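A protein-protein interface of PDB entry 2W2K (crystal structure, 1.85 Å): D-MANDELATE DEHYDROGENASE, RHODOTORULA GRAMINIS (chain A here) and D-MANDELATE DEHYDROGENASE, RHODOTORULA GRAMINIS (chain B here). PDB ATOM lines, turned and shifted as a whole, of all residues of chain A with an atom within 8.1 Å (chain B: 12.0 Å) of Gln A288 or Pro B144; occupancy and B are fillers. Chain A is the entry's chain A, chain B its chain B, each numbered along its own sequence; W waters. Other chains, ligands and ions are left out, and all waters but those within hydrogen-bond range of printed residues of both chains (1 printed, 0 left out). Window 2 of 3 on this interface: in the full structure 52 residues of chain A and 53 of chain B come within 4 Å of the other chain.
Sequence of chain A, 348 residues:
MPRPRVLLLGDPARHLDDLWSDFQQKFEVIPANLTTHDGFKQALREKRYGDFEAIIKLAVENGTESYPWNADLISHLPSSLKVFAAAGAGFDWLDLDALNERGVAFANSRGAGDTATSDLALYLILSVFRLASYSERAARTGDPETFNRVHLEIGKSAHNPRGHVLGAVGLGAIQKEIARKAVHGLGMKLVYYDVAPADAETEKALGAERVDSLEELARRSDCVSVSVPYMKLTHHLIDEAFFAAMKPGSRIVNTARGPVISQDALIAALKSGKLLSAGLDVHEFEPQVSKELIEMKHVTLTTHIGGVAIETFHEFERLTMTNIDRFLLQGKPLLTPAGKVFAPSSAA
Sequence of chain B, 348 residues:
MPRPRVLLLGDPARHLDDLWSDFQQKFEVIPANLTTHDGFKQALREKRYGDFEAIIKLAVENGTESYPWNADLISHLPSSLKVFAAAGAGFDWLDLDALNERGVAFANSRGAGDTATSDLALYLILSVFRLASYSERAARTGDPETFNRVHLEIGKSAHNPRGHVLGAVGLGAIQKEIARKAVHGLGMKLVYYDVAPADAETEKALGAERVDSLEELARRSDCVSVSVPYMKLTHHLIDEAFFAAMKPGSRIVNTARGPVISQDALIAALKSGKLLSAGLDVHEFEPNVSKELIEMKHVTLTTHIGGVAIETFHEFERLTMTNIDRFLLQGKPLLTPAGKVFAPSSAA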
ATOM      1  N   GLN A 263     -13.869  22.447  29.695  1.00  0.00           N
ATOM      2  CA  GLN A 263     -15.258  21.958  29.735  1.00  0.00           C
ATOM      3  C   GLN A 263     -16.118  22.688  30.773  1.00  0.00           C
ATOM      4  O   GLN A 263     -17.270  23.022  30.496  1.00  0.00           O
ATOM      5  CB  GLN A 263     -15.285  20.434  29.980  1.00  0.00           C
ATOM      6  CG  GLN A 263     -16.657  19.809  30.272  1.00  0.00           C
ATOM      7  CD  GLN A 263     -16.678  18.284  30.115  1.00  0.00           C
ATOM      8  OE1 GLN A 263     -16.433  17.756  29.023  1.00  0.00           O
ATOM      9  NE2 GLN A 263     -17.039  17.575  31.193  1.00  0.00           N
ATOM     10  N   VAL A 282     -14.406  17.620  19.378  1.00  0.00           N
ATOM     11  CA  VAL A 282     -13.366  17.097  20.308  1.00  0.00           C
ATOM     12  C   VAL A 282     -13.741  17.437  21.783  1.00  0.00           C
ATOM     13  O   VAL A 282     -14.332  18.490  22.041  1.00  0.00           O
ATOM     14  CB  VAL A 282     -11.930  17.586  19.903  1.00  0.00           C
ATOM     15  CG1 VAL A 282     -11.516  17.033  18.528  1.00  0.00           C
ATOM     16  CG2 VAL A 282     -11.825  19.113  19.887  1.00  0.00           C
ATOM     17  N   HIS A 283     -13.410  16.550  22.730  1.00  0.00           N
ATOM     18  CA  HIS A 283     -14.000  16.587  24.095  1.00  0.00           C
ATOM     19  C   HIS A 283     -12.930  16.465  25.191  1.00  0.00           C
ATOM     20  O   HIS A 283     -11.992  15.669  25.046  1.00  0.00           O
ATOM     21  CB  HIS A 283     -15.055  15.475  24.228  1.00  0.00           C
ATOM     22  CG  HIS A 283     -16.130  15.544  23.179  1.00  0.00           C
ATOM     23  ND1 HIS A 283     -16.001  14.957  21.933  1.00  0.00           N
ATOM     24  CD2 HIS A 283     -17.328  16.185  23.173  1.00  0.00           C
ATOM     25  CE1 HIS A 283     -17.081  15.223  21.211  1.00  0.00           C
ATOM     26  NE2 HIS A 283     -17.897  15.970  21.940  1.00  0.00           N
ATOM     27  N   GLU A 284     -13.049  17.270  26.260  1.00  0.00           N
ATOM     28  CA  GLU A 284     -11.986  17.310  27.304  1.00  0.00           C
ATOM     29  C   GLU A 284     -11.642  15.917  27.861  1.00  0.00           C
ATOM     30  O   GLU A 284     -10.455  15.600  28.030  1.00  0.00           O
ATOM     31  CB  GLU A 284     -12.289  18.310  28.455  1.00  0.00           C
ATOM     32  CG  GLU A 284     -11.126  18.334  29.502  1.00  0.00           C
ATOM     33  CD  GLU A 284     -11.088  19.552  30.447  1.00  0.00           C
ATOM     34  OE1 GLU A 284     -12.069  20.320  30.513  1.00  0.00           O
ATOM     35  OE2 GLU A 284     -10.053  19.718  31.155  1.00  0.00           O
ATOM     36  N   PHE A 285     -12.668  15.115  28.132  1.00  0.00           N
ATOM     37  CA  PHE A 285     -12.513  13.752  28.706  1.00  0.00           C
ATOM     38  C   PHE A 285     -12.870  12.628  27.716  1.00  0.00           C
ATOM     39  O   PHE A 285     -13.330  11.544  28.116  1.00  0.00           O
ATOM     40  CB  PHE A 285     -13.301  13.643  30.024  1.00  0.00           C
ATOM     41  CG  PHE A 285     -12.969  14.742  30.995  1.00  0.00           C
ATOM     42  CD1 PHE A 285     -13.830  15.819  31.176  1.00  0.00           C
ATOM     43  CD2 PHE A 285     -11.758  14.729  31.697  1.00  0.00           C
ATOM     44  CE1 PHE A 285     -13.509  16.856  32.049  1.00  0.00           C
ATOM     45  CE2 PHE A 285     -11.425  15.769  32.570  1.00  0.00           C
ATOM     46  CZ  PHE A 285     -12.309  16.831  32.748  1.00  0.00           C
ATOM     47  N   GLU A 286     -12.641  12.903  26.422  1.00  0.00           N
ATOM     48  CA  GLU A 286     -12.861  11.949  25.321  1.00  0.00           C
ATOM     49  C   GLU A 286     -12.265  10.566  25.662  1.00  0.00           C
ATOM     50  O   GLU A 286     -11.108  10.502  26.088  1.00  0.00           O
ATOM     51  CB  GLU A 286     -12.213  12.513  24.046  1.00  0.00           C
ATOM     52  CG  GLU A 286     -12.720  11.953  22.704  1.00  0.00           C
ATOM     53  CD  GLU A 286     -12.178  12.740  21.511  1.00  0.00           C
ATOM     54  OE1 GLU A 286     -11.577  12.104  20.620  1.00  0.00           O
ATOM     55  OE2 GLU A 286     -12.318  13.998  21.460  1.00  0.00           O
ATOM     56  N   PRO A 287     -13.028   9.461  25.452  1.00  0.00           N
ATOM     57  CA  PRO A 287     -14.323   9.302  24.779  1.00  0.00           C
ATOM     58  C   PRO A 287     -15.585   9.499  25.631  1.00  0.00           C
ATOM     59  O   PRO A 287     -16.663   9.115  25.201  1.00  0.00           O
ATOM     60  CB  PRO A 287     -14.260   7.844  24.270  1.00  0.00           C
ATOM     61  CG  PRO A 287     -13.493   7.131  25.360  1.00  0.00           C
ATOM     62  CD  PRO A 287     -12.506   8.145  25.910  1.00  0.00           C
ATOM     63  N   GLN A 288     -15.459  10.097  26.819  1.00  0.00           N
ATOM     64  CA  GLN A 288     -16.633  10.471  27.623  1.00  0.00           C
ATOM     65  C   GLN A 288     -17.114  11.882  27.280  1.00  0.00           C
ATOM     66  O   GLN A 288     -16.452  12.867  27.637  1.00  0.00           O
ATOM     67  CB  GLN A 288     -16.337  10.367  29.147  1.00  0.00           C
ATOM     68  CG  GLN A 288     -17.571  10.608  30.052  1.00  0.00           C
ATOM     69  CD  GLN A 288     -18.716   9.640  29.794  1.00  0.00           C
ATOM     70  OE1 GLN A 288     -18.609   8.445  30.096  1.00  0.00           O
ATOM     71  NE2 GLN A 288     -19.826  10.146  29.223  1.00  0.00           N
ATOM     72  N   VAL A 289     -18.249  11.964  26.575  1.00  0.00           N
ATOM     73  CA  VAL A 289     -18.919  13.247  26.265  1.00  0.00           C
ATOM     74  C   VAL A 289     -19.647  13.760  27.529  1.00  0.00           C
ATOM     75  O   VAL A 289     -20.187  12.963  28.308  1.00  0.00           O
ATOM     76  CB  VAL A 289     -19.900  13.099  25.055  1.00  0.00           C
ATOM     77  CG1 VAL A 289     -20.741  14.391  24.798  1.00  0.00           C
ATOM     78  CG2 VAL A 289     -19.108  12.708  23.778  1.00  0.00           C
ATOM     79  N   SER A 290     -19.652  15.077  27.720  1.00  0.00           N
ATOM     80  CA  SER A 290     -20.312  15.718  28.887  1.00  0.00           C
ATOM     81  C   SER A 290     -21.837  15.530  28.929  1.00  0.00           C
ATOM     82  O   SER A 290     -22.556  15.984  28.023  1.00  0.00           O
ATOM     83  CB  SER A 290     -19.942  17.212  28.956  1.00  0.00           C
ATOM     84  OG  SER A 290     -20.717  17.906  29.935  1.00  0.00           O
ATOM     85  N   LYS A 291     -22.338  14.880  29.986  1.00  0.00           N
ATOM     86  CA  LYS A 291     -23.795  14.696  30.163  1.00  0.00           C
ATOM     87  C   LYS A 291     -24.539  16.017  30.400  1.00  0.00           C
ATOM     88  O   LYS A 291     -25.699  16.171  29.991  1.00  0.00           O
ATOM     89  CB  LYS A 291     -24.116  13.699  31.287  1.00  0.00           C
ATOM     90  N   ILE A 294     -24.875  17.475  26.864  1.00  0.00           N
ATOM     91  CA  ILE A 294     -25.935  16.698  26.208  1.00  0.00           C
ATOM     92  C   ILE A 294     -27.341  17.183  26.602  1.00  0.00           C
ATOM     93  O   ILE A 294     -28.198  17.341  25.736  1.00  0.00           O
ATOM     94  CB  ILE A 294     -25.795  15.149  26.485  1.00  0.00           C
ATOM     95  CG1 ILE A 294     -24.599  14.552  25.714  1.00  0.00           C
ATOM     96  CG2 ILE A 294     -27.095  14.413  26.114  1.00  0.00           C
ATOM     97  CD1 ILE A 294     -24.069  13.167  26.232  1.00  0.00           C
ATOM     98  N   THR A 303     -18.652  12.730  17.110  1.00  0.00           N
ATOM     99  CA  THR A 303     -17.655  11.734  17.595  1.00  0.00           C
ATOM    100  C   THR A 303     -16.229  11.841  16.994  1.00  0.00           C
ATOM    101  O   THR A 303     -15.714  10.875  16.411  1.00  0.00           O
ATOM    102  CB  THR A 303     -18.188  10.272  17.459  1.00  0.00           C
ATOM    103  OG1 THR A 303     -18.418   9.972  16.074  1.00  0.00           O
ATOM    104  CG2 THR A 303     -19.523  10.064  18.238  1.00  0.00           C
ATOM    105  N   SER B 135     -23.443  10.413  13.655  1.00  0.00           N
ATOM    106  CA  SER B 135     -22.412  10.776  14.625  1.00  0.00           C
ATOM    107  C   SER B 135     -22.965  11.569  15.830  1.00  0.00           C
ATOM    108  O   SER B 135     -22.573  11.291  16.975  1.00  0.00           O
ATOM    109  CB  SER B 135     -21.270  11.553  13.934  1.00  0.00           C
ATOM    110  OG  SER B 135     -20.135  11.708  14.779  1.00  0.00           O
ATOM    111  N   GLU B 136     -23.856  12.545  15.585  1.00  0.00           N
ATOM    112  CA  GLU B 136     -24.481  13.305  16.695  1.00  0.00           C
ATOM    113  C   GLU B 136     -25.253  12.369  17.649  1.00  0.00           C
ATOM    114  O   GLU B 136     -25.103  12.447  18.880  1.00  0.00           O
ATOM    115  CB  GLU B 136     -25.405  14.439  16.186  1.00  0.00           C
ATOM    116  CG  GLU B 136     -24.696  15.608  15.464  1.00  0.00           C
ATOM    117  CD  GLU B 136     -25.507  16.942  15.469  1.00  0.00           C
ATOM    118  OE1 GLU B 136     -26.301  17.182  16.408  1.00  0.00           O
ATOM    119  OE2 GLU B 136     -25.325  17.775  14.544  1.00  0.00           O
ATOM    120  N   ARG B 137     -26.069  11.480  17.088  1.00  0.00           N
ATOM    121  CA  ARG B 137     -26.874  10.556  17.928  1.00  0.00           C
ATOM    122  C   ARG B 137     -26.020   9.622  18.797  1.00  0.00           C
ATOM    123  O   ARG B 137     -26.357   9.386  19.968  1.00  0.00           O
ATOM    124  CB  ARG B 137     -27.899   9.785  17.088  1.00  0.00           C
ATOM    125  CG  ARG B 137     -29.034  10.687  16.636  1.00  0.00           C
ATOM    126  CD  ARG B 137     -30.294   9.973  16.157  1.00  0.00           C
ATOM    127  NE  ARG B 137     -30.079   8.870  15.228  1.00  0.00           N
ATOM    128  CZ  ARG B 137     -29.804   8.984  13.930  1.00  0.00           C
ATOM    129  NH1 ARG B 137     -29.655  10.161  13.347  1.00  0.00           N
ATOM    130  NH2 ARG B 137     -29.661   7.894  13.213  1.00  0.00           N
ATOM    131  N   ALA B 138     -24.910   9.131  18.235  1.00  0.00           N
ATOM    132  CA  ALA B 138     -23.906   8.352  18.988  1.00  0.00           C
ATOM    133  C   ALA B 138     -23.252   9.148  20.130  1.00  0.00           C
ATOM    134  O   ALA B 138     -23.095   8.631  21.257  1.00  0.00           O
ATOM    135  CB  ALA B 138     -22.841   7.821  18.045  1.00  0.00           C
ATOM    136  N   ALA B 139     -22.863  10.400  19.851  1.00  0.00           N
ATOM    137  CA  ALA B 139     -22.283  11.266  20.896  1.00  0.00           C
ATOM    138  C   ALA B 139     -23.252  11.496  22.064  1.00  0.00           C
ATOM    139  O   ALA B 139     -22.831  11.514  23.242  1.00  0.00           O
ATOM    140  CB  ALA B 139     -21.835  12.616  20.303  1.00  0.00           C
ATOM    141  N   ARG B 140     -24.540  11.630  21.737  1.00  0.00           N
ATOM    142  CA  ARG B 140     -25.549  11.987  22.740  1.00  0.00           C
ATOM    143  C   ARG B 140     -26.014  10.819  23.629  1.00  0.00           C
ATOM    144  O   ARG B 140     -26.779  11.029  24.586  1.00  0.00           O
ATOM    145  CB  ARG B 140     -26.719  12.739  22.092  1.00  0.00           C
ATOM    146  CG  ARG B 140     -26.290  14.093  21.500  1.00  0.00           C
ATOM    147  CD  ARG B 140     -27.446  14.911  20.921  1.00  0.00           C
ATOM    148  NE  ARG B 140     -27.938  15.900  21.878  1.00  0.00           N
ATOM    149  CZ  ARG B 140     -27.406  17.105  22.072  1.00  0.00           C
ATOM    150  NH1 ARG B 140     -26.347  17.508  21.381  1.00  0.00           N
ATOM    151  NH2 ARG B 140     -27.939  17.913  22.973  1.00  0.00           N
ATOM    152  N   THR B 141     -25.533   9.604  23.339  1.00  0.00           N
ATOM    153  CA  THR B 141     -25.727   8.441  24.240  1.00  0.00           C
ATOM    154  C   THR B 141     -24.921   8.614  25.536  1.00  0.00           C
ATOM    155  O   THR B 141     -25.279   8.059  26.577  1.00  0.00           O
ATOM    156  CB  THR B 141     -25.346   7.043  23.592  1.00  0.00           C
ATOM    157  OG1 THR B 141     -23.930   6.950  23.411  1.00  0.00           O
ATOM    158  CG2 THR B 141     -26.038   6.839  22.253  1.00  0.00           C
ATOM    159  N   GLY B 142     -23.817   9.356  25.462  1.00  0.00           N
ATOM    160  CA  GLY B 142     -22.893   9.492  26.597  1.00  0.00           C
ATOM    161  C   GLY B 142     -22.131   8.225  26.959  1.00  0.00           C
ATOM    162  O   GLY B 142     -21.537   8.149  28.043  1.00  0.00           O
ATOM    163  N   ASP B 143     -22.141   7.239  26.055  1.00  0.00           N
ATOM    164  CA  ASP B 143     -21.475   5.937  26.255  1.00  0.00           C
ATOM    165  C   ASP B 143     -20.147   5.837  25.489  1.00  0.00           C
ATOM    166  O   ASP B 143     -20.151   5.857  24.256  1.00  0.00           O
ATOM    167  CB  ASP B 143     -22.435   4.812  25.819  1.00  0.00           C
ATOM    168  CG  ASP B 143     -21.903   3.401  26.115  1.00  0.00           C
ATOM    169  OD1 ASP B 143     -20.695   3.135  25.965  1.00  0.00           O
ATOM    170  OD2 ASP B 143     -22.731   2.539  26.470  1.00  0.00           O
ATOM    171  N   PRO B 144     -19.007   5.718  26.218  1.00  0.00           N
ATOM    172  CA  PRO B 144     -17.647   5.700  25.630  1.00  0.00           C
ATOM    173  C   PRO B 144     -17.414   4.622  24.559  1.00  0.00           C
ATOM    174  O   PRO B 144     -16.693   4.866  23.574  1.00  0.00           O
ATOM    175  CB  PRO B 144     -16.735   5.442  26.845  1.00  0.00           C
ATOM    176  CG  PRO B 144     -17.516   5.926  28.011  1.00  0.00           C
ATOM    177  CD  PRO B 144     -18.955   5.610  27.696  1.00  0.00           C
ATOM    178  N   GLU B 145     -17.991   3.439  24.756  1.00  0.00           N
ATOM    179  CA  GLU B 145     -17.832   2.354  23.783  1.00  0.00           C
ATOM    180  C   GLU B 145     -18.580   2.639  22.471  1.00  0.00           C
ATOM    181  O   GLU B 145     -18.090   2.291  21.385  1.00  0.00           O
ATOM    182  CB  GLU B 145     -18.304   1.027  24.380  1.00  0.00           C
ATOM    183  CG  GLU B 145     -17.260   0.345  25.269  1.00  0.00           C
ATOM    184  N   THR B 146     -19.768   3.231  22.588  1.00  0.00           N
ATOM    185  CA  THR B 146     -20.554   3.673  21.416  1.00  0.00           C
ATOM    186  C   THR B 146     -19.800   4.779  20.636  1.00  0.00           C
ATOM    187  O   THR B 146     -19.796   4.776  19.394  1.00  0.00           O
ATOM    188  CB  THR B 146     -21.968   4.142  21.807  1.00  0.00           C
ATOM    189  OG1 THR B 146     -22.694   3.071  22.439  1.00  0.00           O
ATOM    190  CG2 THR B 146     -22.777   4.597  20.542  1.00  0.00           C
ATOM    191  N   PHE B 147     -19.147   5.694  21.363  1.00  0.00           N
ATOM    192  CA  PHE B 147     -18.320   6.763  20.767  1.00  0.00           C
ATOM    193  C   PHE B 147     -17.192   6.183  19.880  1.00  0.00           C
ATOM    194  O   PHE B 147     -17.062   6.532  18.704  1.00  0.00           O
ATOM    195  CB  PHE B 147     -17.740   7.659  21.885  1.00  0.00           C
ATOM    196  CG  PHE B 147     -16.985   8.897  21.401  1.00  0.00           C
ATOM    197  CD1 PHE B 147     -17.546  10.169  21.565  1.00  0.00           C
ATOM    198  CD2 PHE B 147     -15.701   8.796  20.838  1.00  0.00           C
ATOM    199  CE1 PHE B 147     -16.852  11.318  21.162  1.00  0.00           C
ATOM    200  CE2 PHE B 147     -14.990   9.934  20.409  1.00  0.00           C
ATOM    201  CZ  PHE B 147     -15.557  11.201  20.581  1.00  0.00           C
ATOM    202  N   ASN B 148     -16.382   5.283  20.432  1.00  0.00           N
ATOM    203  CA  ASN B 148     -15.309   4.674  19.645  1.00  0.00           C
ATOM    204  C   ASN B 148     -15.794   3.811  18.466  1.00  0.00           C
ATOM    205  O   ASN B 148     -15.173   3.796  17.385  1.00  0.00           O
ATOM    206  CB  ASN B 148     -14.346   3.866  20.539  1.00  0.00           C
ATOM    207  CG  ASN B 148     -13.555   4.746  21.512  1.00  0.00           C
ATOM    208  OD1 ASN B 148     -13.213   4.308  22.620  1.00  0.00           O
ATOM    209  ND2 ASN B 148     -13.247   5.971  21.104  1.00  0.00           N
ATOM    210  N   ARG B 149     -16.876   3.073  18.673  1.00  0.00           N
ATOM    211  CA  ARG B 149     -17.366   2.174  17.635  1.00  0.00           C
ATOM    212  C   ARG B 149     -17.881   2.945  16.407  1.00  0.00           C
ATOM    213  O   ARG B 149     -17.590   2.570  15.256  1.00  0.00           O
ATOM    214  CB  ARG B 149     -18.469   1.269  18.181  1.00  0.00           C
ATOM    215  CG  ARG B 149     -19.052   0.287  17.154  1.00  0.00           C
ATOM    216  CD  ARG B 149     -20.074  -0.663  17.773  1.00  0.00           C
ATOM    217  NE  ARG B 149     -21.006  -0.010  18.700  1.00  0.00           N
ATOM    218  CZ  ARG B 149     -22.148   0.592  18.356  1.00  0.00           C
ATOM    219  NH1 ARG B 149     -22.532   0.659  17.087  1.00  0.00           N
ATOM    220  NH2 ARG B 149     -22.915   1.136  19.296  1.00  0.00           N
ATOM    221  N   VAL B 150     -18.645   4.005  16.663  1.00  0.00           N
ATOM    222  CA  VAL B 150     -19.242   4.810  15.571  1.00  0.00           C
ATOM    223  C   VAL B 150     -18.203   5.663  14.826  1.00  0.00           C
ATOM    224  O   VAL B 150     -18.309   5.840  13.608  1.00  0.00           O
ATOM    225  CB  VAL B 150     -20.455   5.628  16.067  1.00  0.00           C
ATOM    226  CG1 VAL B 150     -20.863   6.715  15.047  1.00  0.00           C
ATOM    227  CG2 VAL B 150     -21.632   4.692  16.306  1.00  0.00           C
ATOM    228  N   HIS B 151     -17.185   6.134  15.549  1.00  0.00           N
ATOM    229  CA  HIS B 151     -16.006   6.806  14.971  1.00  0.00           C
ATOM    230  C   HIS B 151     -15.374   5.931  13.881  1.00  0.00           C
ATOM    231  O   HIS B 151     -15.096   6.405  12.767  1.00  0.00           O
ATOM    232  CB  HIS B 151     -14.983   7.134  16.067  1.00  0.00           C
ATOM    233  CG  HIS B 151     -13.738   7.811  15.570  1.00  0.00           C
ATOM    234  ND1 HIS B 151     -12.600   7.117  15.217  1.00  0.00           N
ATOM    235  CD2 HIS B 151     -13.445   9.120  15.395  1.00  0.00           C
ATOM    236  CE1 HIS B 151     -11.670   7.970  14.823  1.00  0.00           C
ATOM    237  NE2 HIS B 151     -12.153   9.194  14.938  1.00  0.00           N
ATOM    238  N   LEU B 152     -15.188   4.647  14.185  1.00  0.00           N
ATOM    239  CA  LEU B 152     -14.602   3.701  13.208  1.00  0.00           C
ATOM    240  C   LEU B 152     -15.567   3.347  12.064  1.00  0.00           C
ATOM    241  O   LEU B 152     -15.161   3.329  10.896  1.00  0.00           O
ATOM    242  CB  LEU B 152     -14.073   2.437  13.901  1.00  0.00           C
ATOM    243  CG  LEU B 152     -12.891   2.649  14.871  1.00  0.00           C
ATOM    244  CD1 LEU B 152     -12.449   1.325  15.487  1.00  0.00           C
ATOM    245  CD2 LEU B 152     -11.680   3.366  14.237  1.00  0.00           C
ATOM    246  N   GLU B 153     -16.837   3.102  12.398  1.00  0.00           N
ATOM    247  CA  GLU B 153     -17.857   2.730  11.416  1.00  0.00           C
ATOM    248  C   GLU B 153     -18.005   3.796  10.305  1.00  0.00           C
ATOM    249  O   GLU B 153     -18.083   3.461   9.109  1.00  0.00           O
ATOM    250  CB  GLU B 153     -19.205   2.473  12.112  1.00  0.00           C
ATOM    251  CG  GLU B 153     -20.327   1.922  11.186  1.00  0.00           C
ATOM    252  CD  GLU B 153     -21.732   1.982  11.801  1.00  0.00           C
ATOM    253  OE1 GLU B 153     -21.864   2.029  13.052  1.00  0.00           O
ATOM    254  OE2 GLU B 153     -22.723   1.965  11.027  1.00  0.00           O
HETATM  255  O   HOH W   1     -20.411   6.746  30.834  1.00  0.00           O
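O of Ile A294 is in hydrogen-bond range of NH2 of Arg B140 (2.8 Å). The side-chain hydroxyl (OG1) of Thr A303 is in hydrogen-bond range of the side-chain hydroxyl (OG) of Ser B135, 2.8 Å away. O of Gly B142 is in hydrogen-bond range of NE2 of Gln A288.
N of His A283 is in hydrogen-bond range of OE2 of Glu A286.
Among the printed residues, merely in contact across the chains: His A283 with Phe B147 (3.8 Å), Glu A286 with Phe B147 (3.6 Å), Pro A287 with Pro B144 (3.6 Å), Pro A287 with Phe B147 (3.8 Å), Pro A287 with Asn B148 (3.8 Å), Gln A288 with Pro B144 (3.4 Å), Val A289 with Ala B139 (3.8 Å), Val A289 with Phe B147 (3.7 Å), Ile A294 with Ala B139 (3.6 Å), Ile A294 with Gly B142 (3.9 Å), Thr A303 with Ala B139 (3.7 Å), Thr A303 with Phe B147 (3.7 Å) and Thr A303 with His B151 (3.0 Å).
Of chain B, only Phe B147 (3.8 Å) comes within 4 Å of His A283. Glu A286 touches one residue of chain B. Pro A287 touches just these residues of chain B: Pro B144 (3.6 Å), Phe B147 (3.8 Å) and Asn B148 (3.8 Å). Printed residues of chain B within 4 Å of Gln A288: Gly B142 and Pro B144. Ser A290 touches none of the printed residues of chain B. Of the printed residues of chain B, Ile A294 touches Ala B139, Arg B140 and Gly B142. Of the printed residues of chain B, Thr A303 touches Ser B135 (2.8 Å), Ala B139 (3.7 Å), Phe B147 (3.7 Å) and His B151 (3.0 Å). Printed residues of chain A within 4 Å of Ser B135: Thr A303 (2.8 Å). Of the printed residues of chain A, Gly B142 touches Gln A288 and Ile A294. Pro B144 touches just these residues of chain A: Pro A287 (3.6 Å) and Gln A288 (3.4 Å). Val B150 touches none of the printed residues of chain A.
Of the 13 printed residues of chain A, 7 touch a printed residue of chain B. Along chain B the printed residues that touch a printed residue of chain A span positions 135 to 151. Among the printed residues, no Asp or Glu carboxylate lies within 4 Å of a Lys or Arg side-chain nitrogen of the other chain.
Water W1 bridges OE1 of Gln A288 (2.6 Å) and O of Gly B142 (3.3 Å).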
